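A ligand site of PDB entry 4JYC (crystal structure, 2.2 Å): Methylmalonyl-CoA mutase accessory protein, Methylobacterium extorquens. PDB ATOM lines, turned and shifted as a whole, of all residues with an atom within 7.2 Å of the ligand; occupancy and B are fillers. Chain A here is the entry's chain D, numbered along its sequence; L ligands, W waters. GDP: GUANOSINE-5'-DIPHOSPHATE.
O of Val 66 lies within hydrogen-bond range of ND2 of Asn 201 (2.9 Å).
The backbone carbonyl oxygen (O) of Gly 65 sits at hydrogen-bond distance from the side-chain amino group (NZ) of Lys 202, 2.9 Å away.
The side-chain hydroxyl of Thr 71 is in hydrogen-bond range of the side-chain amide nitrogen of Asn 201.
The backbone carbonyl oxygen (O) of Ile 240 lies within hydrogen-bond range of the backbone NH (N) of Lys 202.
OG of Ser 241 is in hydrogen-bond range of N of His 244.
OD1 of Asp 204 lies within hydrogen-bond range of OG of Ser 241 (2.9 Å).
O of Ser 241 is in hydrogen-bond range of N of Lys 246 (2.9 Å).
The side-chain amino group of Lys 68 is in salt-bridge range of the side-chain carboxylate of Glu 154 (2.9 Å).
Residues that only touch the ligand: Val 63 (3.8 Å) and Pro 64 (3.8 Å).
Hydrophobic or aromatic side chains that line the ligand: Val 66 and Leu 243.
Within 4 Å of the ligand: Val 63, Pro 64, Gly 65, Val 66, Gly 67, Lys 68, Ser 69, Thr 70, Asn 201, Lys 202, Asp 204, Ser 241, Gly 242 and Leu 243.
Water W4 lies within hydrogen-bond range of an oxygen (O1B) of the ligand (2.6 Å), the guanidinium group (NH1) of Arg 108 (2.9 Å) and the side-chain amino group (NZ) of Lys 68 (3.1 Å).
Water W3 bridges O2B of the ligand (2.6 Å) and N of Gly 65 (3.4 Å).
Water W2 lies within hydrogen-bond range of O3B of the ligand, O of Val 63 and O of Gly 62.
Water W6 bridges the side-chain amino group (NZ) of Lys 202 (2.8 Å) and a nitrogen (N3) of the ligand (3.1 Å).
O3B of the ligand is in hydrogen-bond range of N of Gly 67 (3.0 Å).
The backbone NH (N) of Val 66 lies within hydrogen-bond range of an oxygen (O3B) of the ligand (3.4 Å).
An oxygen (O6) of the ligand lies close to the side-chain amide oxygen (OD1) of Asn 201 (3.2 Å).
NZ of Lys 202 sits at hydrogen-bond distance from O4' of the ligand (3.3 Å).
The backbone NH (N) of Gly 242 lies within hydrogen-bond range of an oxygen (O6) of the ligand.
The backbone NH (N) of Leu 243 sits at hydrogen-bond distance from an oxygen (O6) of the ligand (3.2 Å).
N of Thr 70 sits at hydrogen-bond distance from O2A of the ligand, at 2.9 Å.
OG of Ser 241 is in hydrogen-bond range of O6 of the ligand (2.9 Å).
The side-chain hydroxyl (OG) of Ser 69 sits at hydrogen-bond distance from an oxygen (O2A) of the ligand.
N of Ser 69 lies within hydrogen-bond range of O1B of the ligand (3.0 Å).
An oxygen (O3B) of the ligand is in hydrogen-bond range of the backbone NH (N) of Lys 68 (2.8 Å).
The side-chain carboxylate (OD2) of Asp 204 is in hydrogen-bond range of a nitrogen (N2) of the ligand (2.5 Å).
An oxygen (O2A) of the ligand lies within hydrogen-bond range of the side-chain hydroxyl (OG1) of Thr 70 (2.5 Å).
The backbone NH of Gly 65 sits at hydrogen-bond distance from an oxygen (O2B) of the ligand (2.8 Å).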
ATOM      1  N   GLY A  62     -13.665  -8.779  21.838  1.00  0.00           N
ATOM      2  CA  GLY A  62     -14.638  -9.856  21.951  1.00  0.00           C
ATOM      3  C   GLY A  62     -15.927  -9.287  22.483  1.00  0.00           C
ATOM      4  O   GLY A  62     -15.933  -8.212  23.096  1.00  0.00           O
ATOM      5  N   VAL A  63     -17.010 -10.010  22.271  1.00  0.00           N
ATOM      6  CA  VAL A  63     -18.338  -9.560  22.630  1.00  0.00           C
ATOM      7  C   VAL A  63     -18.385  -9.421  24.147  1.00  0.00           C
ATOM      8  O   VAL A  63     -17.751 -10.214  24.841  1.00  0.00           O
ATOM      9  CB  VAL A  63     -19.425 -10.547  22.080  1.00  0.00           C
ATOM     10  CG1 VAL A  63     -19.397 -11.890  22.806  1.00  0.00           C
ATOM     11  CG2 VAL A  63     -20.831  -9.958  22.152  1.00  0.00           C
ATOM     12  N   PRO A  64     -19.119  -8.420  24.672  1.00  0.00           N
ATOM     13  CA  PRO A  64     -19.347  -8.347  26.124  1.00  0.00           C
ATOM     14  C   PRO A  64     -19.880  -9.645  26.737  1.00  0.00           C
ATOM     15  O   PRO A  64     -20.801 -10.245  26.213  1.00  0.00           O
ATOM     16  CB  PRO A  64     -20.388  -7.226  26.247  1.00  0.00           C
ATOM     17  CG  PRO A  64     -20.116  -6.362  25.073  1.00  0.00           C
ATOM     18  CD  PRO A  64     -19.780  -7.308  23.957  1.00  0.00           C
ATOM     19  N   GLY A  65     -19.285 -10.080  27.845  1.00  0.00           N
ATOM     20  CA  GLY A  65     -19.588 -11.366  28.454  1.00  0.00           C
ATOM     21  C   GLY A  65     -18.747 -12.544  28.012  1.00  0.00           C
ATOM     22  O   GLY A  65     -18.847 -13.621  28.590  1.00  0.00           O
ATOM     23  N   VAL A  66     -17.905 -12.382  26.994  1.00  0.00           N
ATOM     24  CA  VAL A  66     -17.054 -13.486  26.500  1.00  0.00           C
ATOM     25  C   VAL A  66     -15.966 -13.869  27.534  1.00  0.00           C
ATOM     26  O   VAL A  66     -15.448 -15.008  27.508  1.00  0.00           O
ATOM     27  CB  VAL A  66     -16.384 -13.138  25.147  1.00  0.00           C
ATOM     28  CG1 VAL A  66     -15.244 -12.162  25.330  1.00  0.00           C
ATOM     29  CG2 VAL A  66     -15.922 -14.379  24.419  1.00  0.00           C
ATOM     30  N   GLY A  67     -15.652 -12.918  28.410  1.00  0.00           N
ATOM     31  CA  GLY A  67     -14.627 -13.096  29.454  1.00  0.00           C
ATOM     32  C   GLY A  67     -13.334 -12.301  29.223  1.00  0.00           C
ATOM     33  O   GLY A  67     -12.261 -12.690  29.674  1.00  0.00           O
ATOM     34  N   LYS A  68     -13.421 -11.189  28.500  1.00  0.00           N
ATOM     35  CA  LYS A  68     -12.213 -10.442  28.147  1.00  0.00           C
ATOM     36  C   LYS A  68     -11.505  -9.889  29.385  1.00  0.00           C
ATOM     37  O   LYS A  68     -10.289 -10.064  29.562  1.00  0.00           O
ATOM     38  CB  LYS A  68     -12.536  -9.331  27.158  1.00  0.00           C
ATOM     39  CG  LYS A  68     -11.343  -8.445  26.804  1.00  0.00           C
ATOM     40  CD  LYS A  68     -11.564  -7.715  25.493  1.00  0.00           C
ATOM     41  CE  LYS A  68     -12.807  -6.835  25.475  1.00  0.00           C
ATOM     42  NZ  LYS A  68     -12.835  -5.774  26.550  1.00  0.00           N
ATOM     43  N   SER A  69     -12.250  -9.253  30.268  1.00  0.00           N
ATOM     44  CA  SER A  69     -11.607  -8.605  31.403  1.00  0.00           C
ATOM     45  C   SER A  69     -11.003  -9.641  32.331  1.00  0.00           C
ATOM     46  O   SER A  69      -9.920  -9.433  32.875  1.00  0.00           O
ATOM     47  CB  SER A  69     -12.559  -7.669  32.138  1.00  0.00           C
ATOM     48  OG  SER A  69     -13.248  -8.349  33.135  1.00  0.00           O
ATOM     49  N   THR A  70     -11.657 -10.786  32.461  1.00  0.00           N
ATOM     50  CA  THR A  70     -11.091 -11.891  33.231  1.00  0.00           C
ATOM     51  C   THR A  70      -9.836 -12.477  32.542  1.00  0.00           C
ATOM     52  O   THR A  70      -8.881 -12.815  33.203  1.00  0.00           O
ATOM     53  CB  THR A  70     -12.106 -13.024  33.399  1.00  0.00           C
ATOM     54  OG1 THR A  70     -13.335 -12.472  33.876  1.00  0.00           O
ATOM     55  CG2 THR A  70     -11.596 -14.062  34.403  1.00  0.00           C
ATOM     56  N   THR A  71      -9.868 -12.584  31.225  1.00  0.00           N
ATOM     57  CA  THR A  71      -8.721 -13.140  30.486  1.00  0.00           C
ATOM     58  C   THR A  71      -7.485 -12.200  30.521  1.00  0.00           C
ATOM     59  O   THR A  71      -6.338 -12.633  30.666  1.00  0.00           O
ATOM     60  CB  THR A  71      -9.166 -13.460  29.059  1.00  0.00           C
ATOM     61  OG1 THR A  71     -10.172 -14.506  29.093  1.00  0.00           O
ATOM     62  CG2 THR A  71      -7.997 -13.890  28.187  1.00  0.00           C
ATOM     63  N   ILE A  72      -7.725 -10.907  30.430  1.00  0.00           N
ATOM     64  CA  ILE A  72      -6.660  -9.928  30.466  1.00  0.00           C
ATOM     65  C   ILE A  72      -6.060  -9.880  31.870  1.00  0.00           C
ATOM     66  O   ILE A  72      -4.836  -9.783  32.032  1.00  0.00           O
ATOM     67  CB  ILE A  72      -7.228  -8.562  30.023  1.00  0.00           C
ATOM     68  CG1 ILE A  72      -7.448  -8.545  28.510  1.00  0.00           C
ATOM     69  CG2 ILE A  72      -6.328  -7.387  30.412  1.00  0.00           C
ATOM     70  CD1 ILE A  72      -8.106  -7.266  28.042  1.00  0.00           C
ATOM     71  N   ARG A 108     -12.057  -3.733  37.583  1.00  0.00           N
ATOM     72  CA  ARG A 108     -12.700  -4.991  37.209  1.00  0.00           C
ATOM     73  C   ARG A 108     -11.647  -6.092  37.001  1.00  0.00           C
ATOM     74  O   ARG A 108     -11.964  -7.288  37.121  1.00  0.00           O
ATOM     75  CB  ARG A 108     -13.547  -4.813  35.953  1.00  0.00           C
ATOM     76  CG  ARG A 108     -12.811  -4.140  34.798  1.00  0.00           C
ATOM     77  CD  ARG A 108     -13.638  -4.075  33.531  1.00  0.00           C
ATOM     78  NE  ARG A 108     -12.946  -3.201  32.577  1.00  0.00           N
ATOM     79  CZ  ARG A 108     -12.534  -3.531  31.350  1.00  0.00           C
ATOM     80  NH1 ARG A 108     -12.763  -4.727  30.823  1.00  0.00           N
ATOM     81  NH2 ARG A 108     -11.884  -2.609  30.638  1.00  0.00           N
ATOM     82  N   GLU A 154      -7.753  -2.815  24.579  1.00  0.00           N
ATOM     83  CA  GLU A 154      -9.024  -3.531  24.462  1.00  0.00           C
ATOM     84  C   GLU A 154     -10.146  -2.677  23.918  1.00  0.00           C
ATOM     85  O   GLU A 154     -10.276  -1.492  24.266  1.00  0.00           O
ATOM     86  CB  GLU A 154      -9.453  -4.097  25.815  1.00  0.00           C
ATOM     87  CG  GLU A 154      -9.405  -3.091  26.945  1.00  0.00           C
ATOM     88  CD  GLU A 154      -9.991  -3.625  28.223  1.00  0.00           C
ATOM     89  OE1 GLU A 154     -10.684  -4.657  28.157  1.00  0.00           O
ATOM     90  OE2 GLU A 154      -9.793  -2.986  29.292  1.00  0.00           O
ATOM     91  N   LEU A 175     -11.249 -12.867  21.101  1.00  0.00           N
ATOM     92  CA  LEU A 175     -11.785 -13.838  22.014  1.00  0.00           C
ATOM     93  C   LEU A 175     -13.198 -14.187  21.534  1.00  0.00           C
ATOM     94  O   LEU A 175     -13.952 -13.305  21.122  1.00  0.00           O
ATOM     95  CB  LEU A 175     -11.845 -13.281  23.445  1.00  0.00           C
ATOM     96  CG  LEU A 175     -10.528 -12.676  23.972  1.00  0.00           C
ATOM     97  CD1 LEU A 175     -10.663 -12.240  25.426  1.00  0.00           C
ATOM     98  CD2 LEU A 175      -9.347 -13.598  23.808  1.00  0.00           C
ATOM     99  N   ASN A 201     -12.818 -18.959  24.478  1.00  0.00           N
ATOM    100  CA  ASN A 201     -12.696 -18.906  25.917  1.00  0.00           C
ATOM    101  C   ASN A 201     -13.789 -19.766  26.576  1.00  0.00           C
ATOM    102  O   ASN A 201     -14.661 -20.278  25.910  1.00  0.00           O
ATOM    103  CB  ASN A 201     -12.790 -17.451  26.399  1.00  0.00           C
ATOM    104  CG  ASN A 201     -12.411 -17.262  27.865  1.00  0.00           C
ATOM    105  OD1 ASN A 201     -11.540 -17.949  28.399  1.00  0.00           O
ATOM    106  ND2 ASN A 201     -13.059 -16.332  28.505  1.00  0.00           N
ATOM    107  N   LYS A 202     -13.693 -19.913  27.892  1.00  0.00           N
ATOM    108  CA  LYS A 202     -14.569 -20.819  28.672  1.00  0.00           C
ATOM    109  C   LYS A 202     -14.353 -22.293  28.342  1.00  0.00           C
ATOM    110  O   LYS A 202     -15.240 -23.131  28.519  1.00  0.00           O
ATOM    111  CB  LYS A 202     -16.032 -20.393  28.582  1.00  0.00           C
ATOM    112  CG  LYS A 202     -16.190 -18.890  28.770  1.00  0.00           C
ATOM    113  CD  LYS A 202     -17.620 -18.438  29.033  1.00  0.00           C
ATOM    114  CE  LYS A 202     -17.648 -16.920  29.144  1.00  0.00           C
ATOM    115  NZ  LYS A 202     -18.956 -16.360  29.605  1.00  0.00           N
ATOM    116  N   ALA A 203     -13.129 -22.641  27.972  1.00  0.00           N
ATOM    117  CA  ALA A 203     -12.767 -24.048  27.727  1.00  0.00           C
ATOM    118  C   ALA A 203     -12.488 -24.758  29.056  1.00  0.00           C
ATOM    119  O   ALA A 203     -11.436 -25.377  29.237  1.00  0.00           O
ATOM    120  CB  ALA A 203     -11.564 -24.114  26.815  1.00  0.00           C
ATOM    121  N   ASP A 204     -13.425 -24.662  30.005  1.00  0.00           N
ATOM    122  CA  ASP A 204     -13.202 -25.163  31.356  1.00  0.00           C
ATOM    123  C   ASP A 204     -13.091 -26.694  31.408  1.00  0.00           C
ATOM    124  O   ASP A 204     -13.407 -27.383  30.440  1.00  0.00           O
ATOM    125  CB  ASP A 204     -14.358 -24.754  32.272  1.00  0.00           C
ATOM    126  CG  ASP A 204     -14.497 -23.248  32.413  1.00  0.00           C
ATOM    127  OD1 ASP A 204     -13.652 -22.472  31.893  1.00  0.00           O
ATOM    128  OD2 ASP A 204     -15.488 -22.846  33.057  1.00  0.00           O
ATOM    129  N   ILE A 240      -8.839 -21.327  25.451  1.00  0.00           N
ATOM    130  CA  ILE A 240      -8.362 -20.891  26.761  1.00  0.00           C
ATOM    131  C   ILE A 240      -9.475 -20.866  27.792  1.00  0.00           C
ATOM    132  O   ILE A 240     -10.666 -20.893  27.461  1.00  0.00           O
ATOM    133  CB  ILE A 240      -7.826 -19.443  26.715  1.00  0.00           C
ATOM    134  CG1 ILE A 240      -8.887 -18.506  26.147  1.00  0.00           C
ATOM    135  CG2 ILE A 240      -6.565 -19.362  25.867  1.00  0.00           C
ATOM    136  CD1 ILE A 240      -8.672 -17.051  26.484  1.00  0.00           C
ATOM    137  N   SER A 241      -9.070 -20.782  29.057  1.00  0.00           N
ATOM    138  CA  SER A 241      -9.987 -20.398  30.108  1.00  0.00           C
ATOM    139  C   SER A 241      -9.364 -19.271  30.902  1.00  0.00           C
ATOM    140  O   SER A 241      -8.452 -19.505  31.696  1.00  0.00           O
ATOM    141  CB  SER A 241     -10.291 -21.559  31.042  1.00  0.00           C
ATOM    142  OG  SER A 241     -11.073 -21.082  32.097  1.00  0.00           O
ATOM    143  N   GLY A 242      -9.848 -18.056  30.659  1.00  0.00           N
ATOM    144  CA  GLY A 242      -9.365 -16.920  31.370  1.00  0.00           C
ATOM    145  C   GLY A 242      -9.609 -17.061  32.837  1.00  0.00           C
ATOM    146  O   GLY A 242      -8.779 -16.659  33.642  1.00  0.00           O
ATOM    147  N   LEU A 243     -10.768 -17.621  33.192  1.00  0.00           N
ATOM    148  CA  LEU A 243     -11.132 -17.768  34.594  1.00  0.00           C
ATOM    149  C   LEU A 243     -10.200 -18.752  35.321  1.00  0.00           C
ATOM    150  O   LEU A 243      -9.736 -18.456  36.406  1.00  0.00           O
ATOM    151  CB  LEU A 243     -12.577 -18.232  34.728  1.00  0.00           C
ATOM    152  CG  LEU A 243     -13.159 -18.382  36.133  1.00  0.00           C
ATOM    153  CD1 LEU A 243     -13.038 -17.097  36.961  1.00  0.00           C
ATOM    154  CD2 LEU A 243     -14.630 -18.794  36.017  1.00  0.00           C
ATOM    155  N   HIS A 244      -9.915 -19.901  34.717  1.00  0.00           N
ATOM    156  CA  HIS A 244      -9.155 -20.932  35.435  1.00  0.00           C
ATOM    157  C   HIS A 244      -7.690 -20.989  35.111  1.00  0.00           C
ATOM    158  O   HIS A 244      -6.997 -21.876  35.578  1.00  0.00           O
ATOM    159  CB  HIS A 244      -9.822 -22.291  35.247  1.00  0.00           C
ATOM    160  CG  HIS A 244     -11.233 -22.329  35.794  1.00  0.00           C
ATOM    161  ND1 HIS A 244     -11.500 -22.213  37.114  1.00  0.00           N
ATOM    162  CD2 HIS A 244     -12.457 -22.399  35.151  1.00  0.00           C
ATOM    163  CE1 HIS A 244     -12.826 -22.233  37.307  1.00  0.00           C
ATOM    164  NE2 HIS A 244     -13.417 -22.343  36.104  1.00  0.00           N
ATOM    165  N   GLY A 245      -7.193 -20.011  34.349  1.00  0.00           N
ATOM    166  CA  GLY A 245      -5.767 -19.937  34.005  1.00  0.00           C
ATOM    167  C   GLY A 245      -5.300 -20.836  32.870  1.00  0.00           C
ATOM    168  O   GLY A 245      -4.104 -21.086  32.722  1.00  0.00           O
ATOM    169  N   LYS A 246      -6.217 -21.262  31.997  1.00  0.00           N
ATOM    170  CA  LYS A 246      -5.922 -22.349  31.066  1.00  0.00           C
ATOM    171  C   LYS A 246      -5.457 -21.849  29.682  1.00  0.00           C
ATOM    172  O   LYS A 246      -6.095 -21.008  29.095  1.00  0.00           O
ATOM    173  CB  LYS A 246      -7.190 -23.192  30.926  1.00  0.00           C
ATOM    174  CG  LYS A 246      -7.042 -24.675  31.138  1.00  0.00           C
ATOM    175  CD  LYS A 246      -8.424 -25.330  31.281  1.00  0.00           C
ATOM    176  CE  LYS A 246      -8.390 -26.790  30.855  1.00  0.00           C
ATOM    177  NZ  LYS A 246      -9.751 -27.389  30.789  1.00  0.00           N
HETATM  178  PB  GDP L   1     -16.244  -9.273  29.540  1.00  0.00           P
HETATM  179  O1B GDP L   1     -15.136  -8.429  30.100  1.00  0.00           O
HETATM  180  O2B GDP L   1     -17.573  -8.617  29.557  1.00  0.00           O
HETATM  181  O3B GDP L   1     -15.949  -9.920  28.184  1.00  0.00           O
HETATM  182  O3A GDP L   1     -16.324 -10.605  30.458  1.00  0.00           O
HETATM  183  PA  GDP L   1     -16.022 -10.759  32.027  1.00  0.00           P
HETATM  184  O1A GDP L   1     -16.691  -9.651  32.792  1.00  0.00           O
HETATM  185  O2A GDP L   1     -14.539 -10.990  32.230  1.00  0.00           O
HETATM  186  O5' GDP L   1     -16.741 -12.159  32.391  1.00  0.00           O
HETATM  187  C5' GDP L   1     -18.139 -12.369  32.222  1.00  0.00           C
HETATM  188  C4' GDP L   1     -18.610 -13.608  32.975  1.00  0.00           C
HETATM  189  O4' GDP L   1     -18.023 -14.793  32.376  1.00  0.00           O
HETATM  190  C3' GDP L   1     -18.222 -13.549  34.452  1.00  0.00           C
HETATM  191  O3' GDP L   1     -19.288 -14.005  35.337  1.00  0.00           O
HETATM  192  C2' GDP L   1     -16.961 -14.398  34.438  1.00  0.00           C
HETATM  193  O2' GDP L   1     -16.632 -14.987  35.681  1.00  0.00           O
HETATM  194  C1' GDP L   1     -17.254 -15.445  33.368  1.00  0.00           C
HETATM  195  N9  GDP L   1     -16.018 -15.964  32.779  1.00  0.00           N
HETATM  196  C8  GDP L   1     -14.956 -15.255  32.320  1.00  0.00           C
HETATM  197  N7  GDP L   1     -14.011 -16.103  31.843  1.00  0.00           N
HETATM  198  C5  GDP L   1     -14.443 -17.365  31.988  1.00  0.00           C
HETATM  199  C6  GDP L   1     -13.931 -18.722  31.677  1.00  0.00           C
HETATM  200  O6  GDP L   1     -12.798 -18.926  31.157  1.00  0.00           O
HETATM  201  N1  GDP L   1     -14.732 -19.734  32.000  1.00  0.00           N
HETATM  202  C2  GDP L   1     -15.955 -19.556  32.567  1.00  0.00           C
HETATM  203  N2  GDP L   1     -16.720 -20.633  32.859  1.00  0.00           N
HETATM  204  N3  GDP L   1     -16.495 -18.368  32.849  1.00  0.00           N
HETATM  205  C4  GDP L   1     -15.783 -17.261  32.603  1.00  0.00           C
HETATM  206  O   HOH W   1     -21.434 -11.327  32.007  1.00  0.00           O
HETATM  207  O   HOH W   2     -15.797  -8.285  26.163  1.00  0.00           O
HETATM  208  O   HOH W   3     -19.806  -8.740  30.889  1.00  0.00           O
HETATM  209  O   HOH W   4     -14.595  -6.118  29.076  1.00  0.00           O
HETATM  210  O   HOH W   5     -16.076  -6.209  32.433  1.00  0.00           O
HETATM  211  O   HOH W   6     -19.405 -17.837  31.955  1.00  0.00           O
